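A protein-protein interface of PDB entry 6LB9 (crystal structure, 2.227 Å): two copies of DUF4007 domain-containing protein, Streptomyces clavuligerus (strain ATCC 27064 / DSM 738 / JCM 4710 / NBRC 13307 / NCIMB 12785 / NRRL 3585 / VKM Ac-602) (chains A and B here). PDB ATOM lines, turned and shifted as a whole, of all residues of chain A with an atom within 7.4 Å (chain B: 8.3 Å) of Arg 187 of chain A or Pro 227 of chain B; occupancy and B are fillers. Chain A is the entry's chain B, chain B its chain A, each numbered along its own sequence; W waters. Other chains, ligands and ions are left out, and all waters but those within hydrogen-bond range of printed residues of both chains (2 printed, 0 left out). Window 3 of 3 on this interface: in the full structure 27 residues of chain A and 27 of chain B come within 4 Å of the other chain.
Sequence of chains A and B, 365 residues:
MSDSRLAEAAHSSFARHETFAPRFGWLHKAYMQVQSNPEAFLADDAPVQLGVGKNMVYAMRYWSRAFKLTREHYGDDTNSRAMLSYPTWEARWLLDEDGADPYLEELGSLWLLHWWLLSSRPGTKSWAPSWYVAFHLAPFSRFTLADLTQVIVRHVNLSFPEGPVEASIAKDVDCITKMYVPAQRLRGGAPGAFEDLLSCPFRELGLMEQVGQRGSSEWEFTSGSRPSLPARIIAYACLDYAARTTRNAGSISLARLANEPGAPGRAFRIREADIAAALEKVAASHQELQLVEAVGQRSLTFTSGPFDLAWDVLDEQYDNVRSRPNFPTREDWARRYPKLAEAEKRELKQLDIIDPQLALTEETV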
ATOM      1  N   PRO A 182      23.896  32.218  -0.994  1.00  0.00           N
ATOM      2  CA  PRO A 182      24.880  31.201  -1.389  1.00  0.00           C
ATOM      3  C   PRO A 182      25.143  31.189  -2.889  1.00  0.00           C
ATOM      4  O   PRO A 182      24.246  31.401  -3.709  1.00  0.00           O
ATOM      5  CB  PRO A 182      24.236  29.888  -0.926  1.00  0.00           C
ATOM      6  CG  PRO A 182      23.339  30.290   0.212  1.00  0.00           C
ATOM      7  CD  PRO A 182      22.814  31.641  -0.169  1.00  0.00           C
ATOM      8  N   ALA A 183      26.400  30.898  -3.233  1.00  0.00           N
ATOM      9  CA  ALA A 183      26.847  30.927  -4.620  1.00  0.00           C
ATOM     10  C   ALA A 183      26.225  29.825  -5.461  1.00  0.00           C
ATOM     11  O   ALA A 183      26.192  29.938  -6.687  1.00  0.00           O
ATOM     12  CB  ALA A 183      28.372  30.820  -4.681  1.00  0.00           C
ATOM     13  N   GLN A 184      25.747  28.750  -4.842  1.00  0.00           N
ATOM     14  CA  GLN A 184      25.040  27.732  -5.611  1.00  0.00           C
ATOM     15  C   GLN A 184      23.753  28.269  -6.221  1.00  0.00           C
ATOM     16  O   GLN A 184      23.237  27.662  -7.168  1.00  0.00           O
ATOM     17  CB  GLN A 184      24.740  26.508  -4.737  1.00  0.00           C
ATOM     18  CG  GLN A 184      25.990  25.709  -4.397  1.00  0.00           C
ATOM     19  CD  GLN A 184      26.985  26.505  -3.550  1.00  0.00           C
ATOM     20  OE1 GLN A 184      28.188  26.532  -3.843  1.00  0.00           O
ATOM     21  NE2 GLN A 184      26.493  27.128  -2.489  1.00  0.00           N
ATOM     22  N   ARG A 185      23.245  29.387  -5.711  1.00  0.00           N
ATOM     23  CA  ARG A 185      22.077  30.077  -6.263  1.00  0.00           C
ATOM     24  C   ARG A 185      22.492  31.293  -7.081  1.00  0.00           C
ATOM     25  O   ARG A 185      22.004  32.395  -6.852  1.00  0.00           O
ATOM     26  CB  ARG A 185      21.134  30.479  -5.138  1.00  0.00           C
ATOM     27  CG  ARG A 185      20.449  29.325  -4.409  1.00  0.00           C
ATOM     28  CD  ARG A 185      21.206  28.892  -3.173  1.00  0.00           C
ATOM     29  NE  ARG A 185      20.282  28.431  -2.138  1.00  0.00           N
ATOM     30  CZ  ARG A 185      19.721  29.235  -1.234  1.00  0.00           C
ATOM     31  NH1 ARG A 185      20.004  30.526  -1.238  1.00  0.00           N
ATOM     32  NH2 ARG A 185      18.881  28.757  -0.320  1.00  0.00           N
ATOM     33  N   LEU A 186      23.421  31.110  -8.017  1.00  0.00           N
ATOM     34  CA  LEU A 186      23.939  32.187  -8.859  1.00  0.00           C
ATOM     35  C   LEU A 186      24.403  31.567 -10.172  1.00  0.00           C
ATOM     36  O   LEU A 186      24.881  30.430 -10.194  1.00  0.00           O
ATOM     37  CB  LEU A 186      25.104  32.953  -8.200  1.00  0.00           C
ATOM     38  CG  LEU A 186      24.970  33.682  -6.844  1.00  0.00           C
ATOM     39  CD1 LEU A 186      26.323  34.188  -6.371  1.00  0.00           C
ATOM     40  CD2 LEU A 186      23.961  34.853  -6.863  1.00  0.00           C
ATOM     41  N   ARG A 187      24.249  32.311 -11.267  1.00  0.00           N
ATOM     42  CA  ARG A 187      24.580  31.818 -12.603  1.00  0.00           C
ATOM     43  C   ARG A 187      25.668  32.697 -13.206  1.00  0.00           C
ATOM     44  O   ARG A 187      25.440  33.889 -13.448  1.00  0.00           O
ATOM     45  CB  ARG A 187      23.339  31.789 -13.504  1.00  0.00           C
ATOM     46  CG  ARG A 187      22.146  31.020 -12.918  1.00  0.00           C
ATOM     47  CD  ARG A 187      22.311  29.510 -13.078  1.00  0.00           C
ATOM     48  NE  ARG A 187      22.952  28.898 -11.914  1.00  0.00           N
ATOM     49  CZ  ARG A 187      22.310  28.253 -10.940  1.00  0.00           C
ATOM     50  NH1 ARG A 187      20.992  28.104 -10.982  1.00  0.00           N
ATOM     51  NH2 ARG A 187      22.993  27.739  -9.927  1.00  0.00           N
ATOM     52  N   GLY A 188      26.841  32.107 -13.463  1.00  0.00           N
ATOM     53  CA  GLY A 188      27.987  32.864 -13.944  1.00  0.00           C
ATOM     54  C   GLY A 188      28.470  32.504 -15.337  1.00  0.00           C
ATOM     55  O   GLY A 188      29.640  32.145 -15.513  1.00  0.00           O
ATOM     56  N   GLY A 189      27.586  32.605 -16.329  1.00  0.00           N
ATOM     57  CA  GLY A 189      27.931  32.366 -17.726  1.00  0.00           C
ATOM     58  C   GLY A 189      28.740  31.112 -18.022  1.00  0.00           C
ATOM     59  O   GLY A 189      28.286  30.201 -18.721  1.00  0.00           O
ATOM     60  N   GLU A 195      36.246  30.374 -14.409  1.00  0.00           N
ATOM     61  CA  GLU A 195      34.834  30.712 -14.400  1.00  0.00           C
ATOM     62  C   GLU A 195      34.658  31.874 -13.436  1.00  0.00           C
ATOM     63  O   GLU A 195      35.505  32.120 -12.584  1.00  0.00           O
ATOM     64  CB  GLU A 195      33.969  29.521 -14.009  1.00  0.00           C
ATOM     65  N   ASP A 196      33.552  32.602 -13.573  1.00  0.00           N
ATOM     66  CA  ASP A 196      33.520  33.931 -12.976  1.00  0.00           C
ATOM     67  C   ASP A 196      33.412  33.909 -11.450  1.00  0.00           C
ATOM     68  O   ASP A 196      33.917  34.834 -10.806  1.00  0.00           O
ATOM     69  CB  ASP A 196      32.389  34.762 -13.581  1.00  0.00           C
ATOM     70  CG  ASP A 196      32.397  34.728 -15.103  1.00  0.00           C
ATOM     71  OD1 ASP A 196      33.086  35.581 -15.715  1.00  0.00           O
ATOM     72  OD2 ASP A 196      31.697  33.876 -15.683  1.00  0.00           O
ATOM     73  N   LEU A 197      32.789  32.886 -10.849  1.00  0.00           N
ATOM     74  CA  LEU A 197      32.184  33.087  -9.527  1.00  0.00           C
ATOM     75  C   LEU A 197      33.211  33.400  -8.445  1.00  0.00           C
ATOM     76  O   LEU A 197      34.166  32.645  -8.221  1.00  0.00           O
ATOM     77  CB  LEU A 197      31.324  31.891  -9.111  1.00  0.00           C
ATOM     78  CG  LEU A 197      29.904  31.798  -9.686  1.00  0.00           C
ATOM     79  CD1 LEU A 197      28.992  30.828  -8.874  1.00  0.00           C
ATOM     80  CD2 LEU A 197      29.279  33.177  -9.771  1.00  0.00           C
ATOM     81  N   GLN A 210      17.496  31.909  -1.892  1.00  0.00           N
ATOM     82  CA  GLN A 210      16.610  31.691  -3.029  1.00  0.00           C
ATOM     83  C   GLN A 210      15.362  30.931  -2.570  1.00  0.00           C
ATOM     84  O   GLN A 210      15.408  30.149  -1.619  1.00  0.00           O
ATOM     85  CB  GLN A 210      17.370  30.900  -4.099  1.00  0.00           C
ATOM     86  CG  GLN A 210      16.598  30.426  -5.330  1.00  0.00           C
ATOM     87  CD  GLN A 210      17.482  30.331  -6.562  1.00  0.00           C
ATOM     88  OE1 GLN A 210      17.718  31.318  -7.246  1.00  0.00           O
ATOM     89  NE2 GLN A 210      17.988  29.131  -6.837  1.00  0.00           N
ATOM     90  N   ARG A 214      13.865  26.771  -8.830  1.00  0.00           N
ATOM     91  CA  ARG A 214      14.062  26.307 -10.199  1.00  0.00           C
ATOM     92  C   ARG A 214      15.487  26.541 -10.733  1.00  0.00           C
ATOM     93  O   ARG A 214      15.933  25.759 -11.582  1.00  0.00           O
ATOM     94  CB  ARG A 214      13.043  26.973 -11.126  1.00  0.00           C
ATOM     95  N   GLY A 215      16.235  27.575 -10.305  1.00  0.00           N
ATOM     96  CA  GLY A 215      15.900  28.600  -9.323  1.00  0.00           C
ATOM     97  C   GLY A 215      14.764  29.537  -9.698  1.00  0.00           C
ATOM     98  O   GLY A 215      14.792  30.167 -10.756  1.00  0.00           O
ATOM     99  N   TRP A 219      13.205  35.570  -3.960  1.00  0.00           N
ATOM    100  CA  TRP A 219      14.258  35.542  -2.955  1.00  0.00           C
ATOM    101  C   TRP A 219      13.644  35.952  -1.626  1.00  0.00           C
ATOM    102  O   TRP A 219      12.574  36.558  -1.590  1.00  0.00           O
ATOM    103  CB  TRP A 219      15.399  36.500  -3.307  1.00  0.00           C
ATOM    104  CG  TRP A 219      15.897  36.310  -4.676  1.00  0.00           C
ATOM    105  CD1 TRP A 219      15.329  36.778  -5.830  1.00  0.00           C
ATOM    106  CD2 TRP A 219      17.072  35.605  -5.059  1.00  0.00           C
ATOM    107  NE1 TRP A 219      16.079  36.394  -6.912  1.00  0.00           N
ATOM    108  CE2 TRP A 219      17.161  35.675  -6.464  1.00  0.00           C
ATOM    109  CE3 TRP A 219      18.059  34.911  -4.354  1.00  0.00           C
ATOM    110  CZ2 TRP A 219      18.203  35.081  -7.174  1.00  0.00           C
ATOM    111  CZ3 TRP A 219      19.092  34.324  -5.059  1.00  0.00           C
ATOM    112  CH2 TRP A 219      19.158  34.411  -6.450  1.00  0.00           C
ATOM    113  N   LEU B 107      36.183  31.347  -6.246  1.00  0.00           N
ATOM    114  CA  LEU B 107      35.813  30.079  -5.629  1.00  0.00           C
ATOM    115  C   LEU B 107      36.559  28.896  -6.240  1.00  0.00           C
ATOM    116  O   LEU B 107      36.722  27.874  -5.566  1.00  0.00           O
ATOM    117  CB  LEU B 107      34.299  29.881  -5.714  1.00  0.00           C
ATOM    118  CG  LEU B 107      33.495  30.800  -4.780  1.00  0.00           C
ATOM    119  CD1 LEU B 107      32.009  30.727  -5.083  1.00  0.00           C
ATOM    120  CD2 LEU B 107      33.770  30.443  -3.315  1.00  0.00           C
ATOM    121  N   GLY B 108      37.046  29.016  -7.479  1.00  0.00           N
ATOM    122  CA  GLY B 108      37.874  27.964  -8.052  1.00  0.00           C
ATOM    123  C   GLY B 108      39.150  27.693  -7.269  1.00  0.00           C
ATOM    124  O   GLY B 108      39.656  26.562  -7.257  1.00  0.00           O
ATOM    125  N   TRP B 111      37.984  25.246  -4.506  1.00  0.00           N
ATOM    126  CA  TRP B 111      37.900  23.927  -5.133  1.00  0.00           C
ATOM    127  C   TRP B 111      39.293  23.323  -5.297  1.00  0.00           C
ATOM    128  O   TRP B 111      39.518  22.150  -4.982  1.00  0.00           O
ATOM    129  CB  TRP B 111      37.191  24.027  -6.501  1.00  0.00           C
ATOM    130  CG  TRP B 111      35.694  24.215  -6.384  1.00  0.00           C
ATOM    131  CD1 TRP B 111      34.994  25.358  -6.638  1.00  0.00           C
ATOM    132  CD2 TRP B 111      34.728  23.251  -5.929  1.00  0.00           C
ATOM    133  NE1 TRP B 111      33.661  25.165  -6.392  1.00  0.00           N
ATOM    134  CE2 TRP B 111      33.468  23.887  -5.942  1.00  0.00           C
ATOM    135  CE3 TRP B 111      34.807  21.922  -5.503  1.00  0.00           C
ATOM    136  CZ2 TRP B 111      32.294  23.239  -5.562  1.00  0.00           C
ATOM    137  CZ3 TRP B 111      33.628  21.275  -5.118  1.00  0.00           C
ATOM    138  CH2 TRP B 111      32.396  21.933  -5.158  1.00  0.00           C
ATOM    139  N   LEU B 205      31.652  26.106  -0.913  1.00  0.00           N
ATOM    140  CA  LEU B 205      31.591  25.092  -1.958  1.00  0.00           C
ATOM    141  C   LEU B 205      30.292  24.286  -1.926  1.00  0.00           C
ATOM    142  O   LEU B 205      30.051  23.512  -2.853  1.00  0.00           O
ATOM    143  CB  LEU B 205      32.795  24.142  -1.842  1.00  0.00           C
ATOM    144  CG  LEU B 205      34.214  24.733  -1.850  1.00  0.00           C
ATOM    145  CD1 LEU B 205      35.243  23.618  -1.810  1.00  0.00           C
ATOM    146  CD2 LEU B 205      34.424  25.622  -3.080  1.00  0.00           C
ATOM    147  N   GLY B 224      23.912  18.350  -5.992  1.00  0.00           N
ATOM    148  CA  GLY B 224      23.408  19.194  -7.057  1.00  0.00           C
ATOM    149  C   GLY B 224      24.478  19.611  -8.058  1.00  0.00           C
ATOM    150  O   GLY B 224      25.586  19.074  -8.107  1.00  0.00           O
ATOM    151  N   SER B 225      24.116  20.598  -8.878  1.00  0.00           N
ATOM    152  CA  SER B 225      25.024  21.207  -9.838  1.00  0.00           C
ATOM    153  C   SER B 225      26.056  22.080  -9.112  1.00  0.00           C
ATOM    154  O   SER B 225      25.836  22.531  -7.985  1.00  0.00           O
ATOM    155  CB  SER B 225      24.227  22.048 -10.833  1.00  0.00           C
ATOM    156  OG  SER B 225      24.857  22.053 -12.098  1.00  0.00           O
ATOM    157  N   ARG B 226      27.196  22.328  -9.765  1.00  0.00           N
ATOM    158  CA  ARG B 226      28.296  23.071  -9.144  1.00  0.00           C
ATOM    159  C   ARG B 226      28.673  24.288  -9.975  1.00  0.00           C
ATOM    160  O   ARG B 226      29.770  24.346 -10.546  1.00  0.00           O
ATOM    161  CB  ARG B 226      29.523  22.186  -8.947  1.00  0.00           C
ATOM    162  CG  ARG B 226      29.228  20.860  -8.311  1.00  0.00           C
ATOM    163  CD  ARG B 226      29.338  20.923  -6.819  1.00  0.00           C
ATOM    164  NE  ARG B 226      29.076  19.611  -6.243  1.00  0.00           N
ATOM    165  CZ  ARG B 226      28.273  19.396  -5.206  1.00  0.00           C
ATOM    166  NH1 ARG B 226      27.653  20.415  -4.608  1.00  0.00           N
ATOM    167  NH2 ARG B 226      28.094  18.153  -4.773  1.00  0.00           N
ATOM    168  N   PRO B 227      27.815  25.306 -10.026  1.00  0.00           N
ATOM    169  CA  PRO B 227      28.128  26.483 -10.852  1.00  0.00           C
ATOM    170  C   PRO B 227      29.388  27.238 -10.429  1.00  0.00           C
ATOM    171  O   PRO B 227      29.871  28.068 -11.206  1.00  0.00           O
ATOM    172  CB  PRO B 227      26.879  27.356 -10.697  1.00  0.00           C
ATOM    173  CG  PRO B 227      26.262  26.889  -9.377  1.00  0.00           C
ATOM    174  CD  PRO B 227      26.525  25.434  -9.324  1.00  0.00           C
ATOM    175  N   SER B 228      29.940  26.995  -9.237  1.00  0.00           N
ATOM    176  CA  SER B 228      31.153  27.694  -8.817  1.00  0.00           C
ATOM    177  C   SER B 228      32.431  26.921  -9.151  1.00  0.00           C
ATOM    178  O   SER B 228      33.534  27.414  -8.876  1.00  0.00           O
ATOM    179  CB  SER B 228      31.108  27.983  -7.308  1.00  0.00           C
ATOM    180  OG  SER B 228      31.434  26.827  -6.538  1.00  0.00           O
ATOM    181  N   LEU B 229      32.314  25.721  -9.710  1.00  0.00           N
ATOM    182  CA  LEU B 229      33.479  24.911 -10.035  1.00  0.00           C
ATOM    183  C   LEU B 229      33.888  25.160 -11.490  1.00  0.00           C
ATOM    184  O   LEU B 229      33.262  24.617 -12.403  1.00  0.00           O
ATOM    185  CB  LEU B 229      33.155  23.436  -9.786  1.00  0.00           C
ATOM    186  CG  LEU B 229      34.196  22.382 -10.159  1.00  0.00           C
ATOM    187  CD1 LEU B 229      35.535  22.696  -9.516  1.00  0.00           C
ATOM    188  CD2 LEU B 229      33.717  20.966  -9.794  1.00  0.00           C
ATOM    189  N   PRO B 230      34.906  25.981 -11.748  1.00  0.00           N
ATOM    190  CA  PRO B 230      35.288  26.274 -13.136  1.00  0.00           C
ATOM    191  C   PRO B 230      35.748  25.040 -13.910  1.00  0.00           C
ATOM    192  O   PRO B 230      36.326  24.092 -13.363  1.00  0.00           O
ATOM    193  CB  PRO B 230      36.443  27.275 -12.974  1.00  0.00           C
ATOM    194  CG  PRO B 230      36.297  27.807 -11.551  1.00  0.00           C
ATOM    195  CD  PRO B 230      35.788  26.657 -10.779  1.00  0.00           C
ATOM    196  N   ALA B 231      35.531  25.094 -15.221  1.00  0.00           N
ATOM    197  CA  ALA B 231      35.818  23.951 -16.080  1.00  0.00           C
ATOM    198  C   ALA B 231      37.311  23.648 -16.122  1.00  0.00           C
ATOM    199  O   ALA B 231      37.716  22.478 -16.099  1.00  0.00           O
ATOM    200  CB  ALA B 231      35.269  24.215 -17.483  1.00  0.00           C
ATOM    201  N   ILE B 270      30.753  15.504  -8.402  1.00  0.00           N
ATOM    202  CA  ILE B 270      30.130  15.860  -9.680  1.00  0.00           C
ATOM    203  C   ILE B 270      29.938  14.606 -10.516  1.00  0.00           C
ATOM    204  O   ILE B 270      30.721  13.654 -10.434  1.00  0.00           O
ATOM    205  CB  ILE B 270      30.953  16.891 -10.491  1.00  0.00           C
ATOM    206  CG1 ILE B 270      32.398  16.426 -10.671  1.00  0.00           C
ATOM    207  CG2 ILE B 270      30.935  18.233  -9.837  1.00  0.00           C
ATOM    208  CD1 ILE B 270      33.197  17.388 -11.544  1.00  0.00           C
ATOM    209  N   ASP B 274      28.681  16.087 -16.024  1.00  0.00           N
ATOM    210  CA  ASP B 274      29.301  17.361 -15.656  1.00  0.00           C
ATOM    211  C   ASP B 274      30.798  17.362 -15.966  1.00  0.00           C
ATOM    212  O   ASP B 274      31.344  18.380 -16.405  1.00  0.00           O
ATOM    213  CB  ASP B 274      29.078  17.656 -14.172  1.00  0.00           C
ATOM    214  CG  ASP B 274      27.606  17.829 -13.814  1.00  0.00           C
ATOM    215  OD1 ASP B 274      26.866  18.469 -14.589  1.00  0.00           O
ATOM    216  OD2 ASP B 274      27.195  17.325 -12.743  1.00  0.00           O
HETATM  217  O   HOH W   1      35.593  30.822  -9.455  1.00  0.00           O
HETATM  218  O   HOH W   2      28.759  25.372  -6.624  1.00  0.00           O
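No position is printed for both chains.
NE1 of Trp 111 of chain B is in hydrogen-bond range of OG of Ser 228 of chain B, at 2.8 Å. O of Gln 184 of chain A is in hydrogen-bond range of NH2 of Arg 187 of chain A.
Of the 14 printed residues of chain B, 5 touch a printed residue of chain A. Of the 15 printed residues of chain A, 6 touch a printed residue of chain B. Printed residues of chain A that touch a printed residue of chain B: Ala 183, Gln 184, Leu 186, Arg 187, Glu 195 and Leu 197. Hydrophobic or aromatic side chains of chain A that line the printed part of chain B: Ala 183 and Leu 197. Along chain A the printed residues that touch a printed residue of chain B span positions 183 to 197. Among the printed residues, no Asp or Glu carboxylate lies within 4 Å of a Lys or Arg side-chain nitrogen of the other chain.
O of Leu 197 of chain A sits at hydrogen-bond distance from N of Leu 107 of chain B, at 3.1 Å.
Arg 187 of chain A touches just one residue of chain B: Pro 227. Of the printed residues of chain A, Pro 227 of chain B touches Gln 184, Leu 186, Arg 187 and Leu 197. Of the printed residues of chain B, Leu 186 of chain A touches Pro 227 (3.7 Å). Of the printed residues of chain B, Gln 184 of chain A touches Leu 205 (3.6 Å) and Pro 227 (3.8 Å). Gly 215 of chain A touches none of the printed residues of chain B. Trp 219 of chain A touches none of the printed residues of chain B. The nearest residue of chain B that does not touch Arg 187 of chain A is Ser 225 of chain B (5.9 Å). The nearest printed residue of chain A that does not touch Pro 230 of chain B is Asp 196 of chain A (5.9 Å).
Water W1 lies within hydrogen-bond range of the backbone carbonyl oxygen (O) of Leu 197 of chain A (2.6 Å), the backbone NH (N) of Gly 108 of chain B (3.0 Å), the backbone NH (N) of Leu 107 of chain B (3.3 Å) and the backbone carbonyl oxygen (O) of Glu 195 of chain A (3.4 Å). Water W2 lies within hydrogen-bond range of the side-chain hydroxyl of Ser 228 of chain B (3.0 Å) and the side-chain amide oxygen of Gln 184 of chain A (3.1 Å).
Ala 183 of chain A touches Leu 107 of chain B. Leu 205 of chain B touches Gln 184 of chain A. Gln 184 of chain A touches Pro 227 of chain B (O to CG, 3.8 Å). Leu 186 of chain A touches Pro 227 of chain B. NH2 of Arg 187 of chain A touches CG of Pro 227 of chain B (3.4 Å). Glu 195 of chain A touches Pro 230 of chain B (N to CB, 3.4 Å). Leu 197 of chain A touches Pro 227 of chain B (CD1 to O, 3.7 Å). Ser 228 of chain B touches Leu 197 of chain A.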
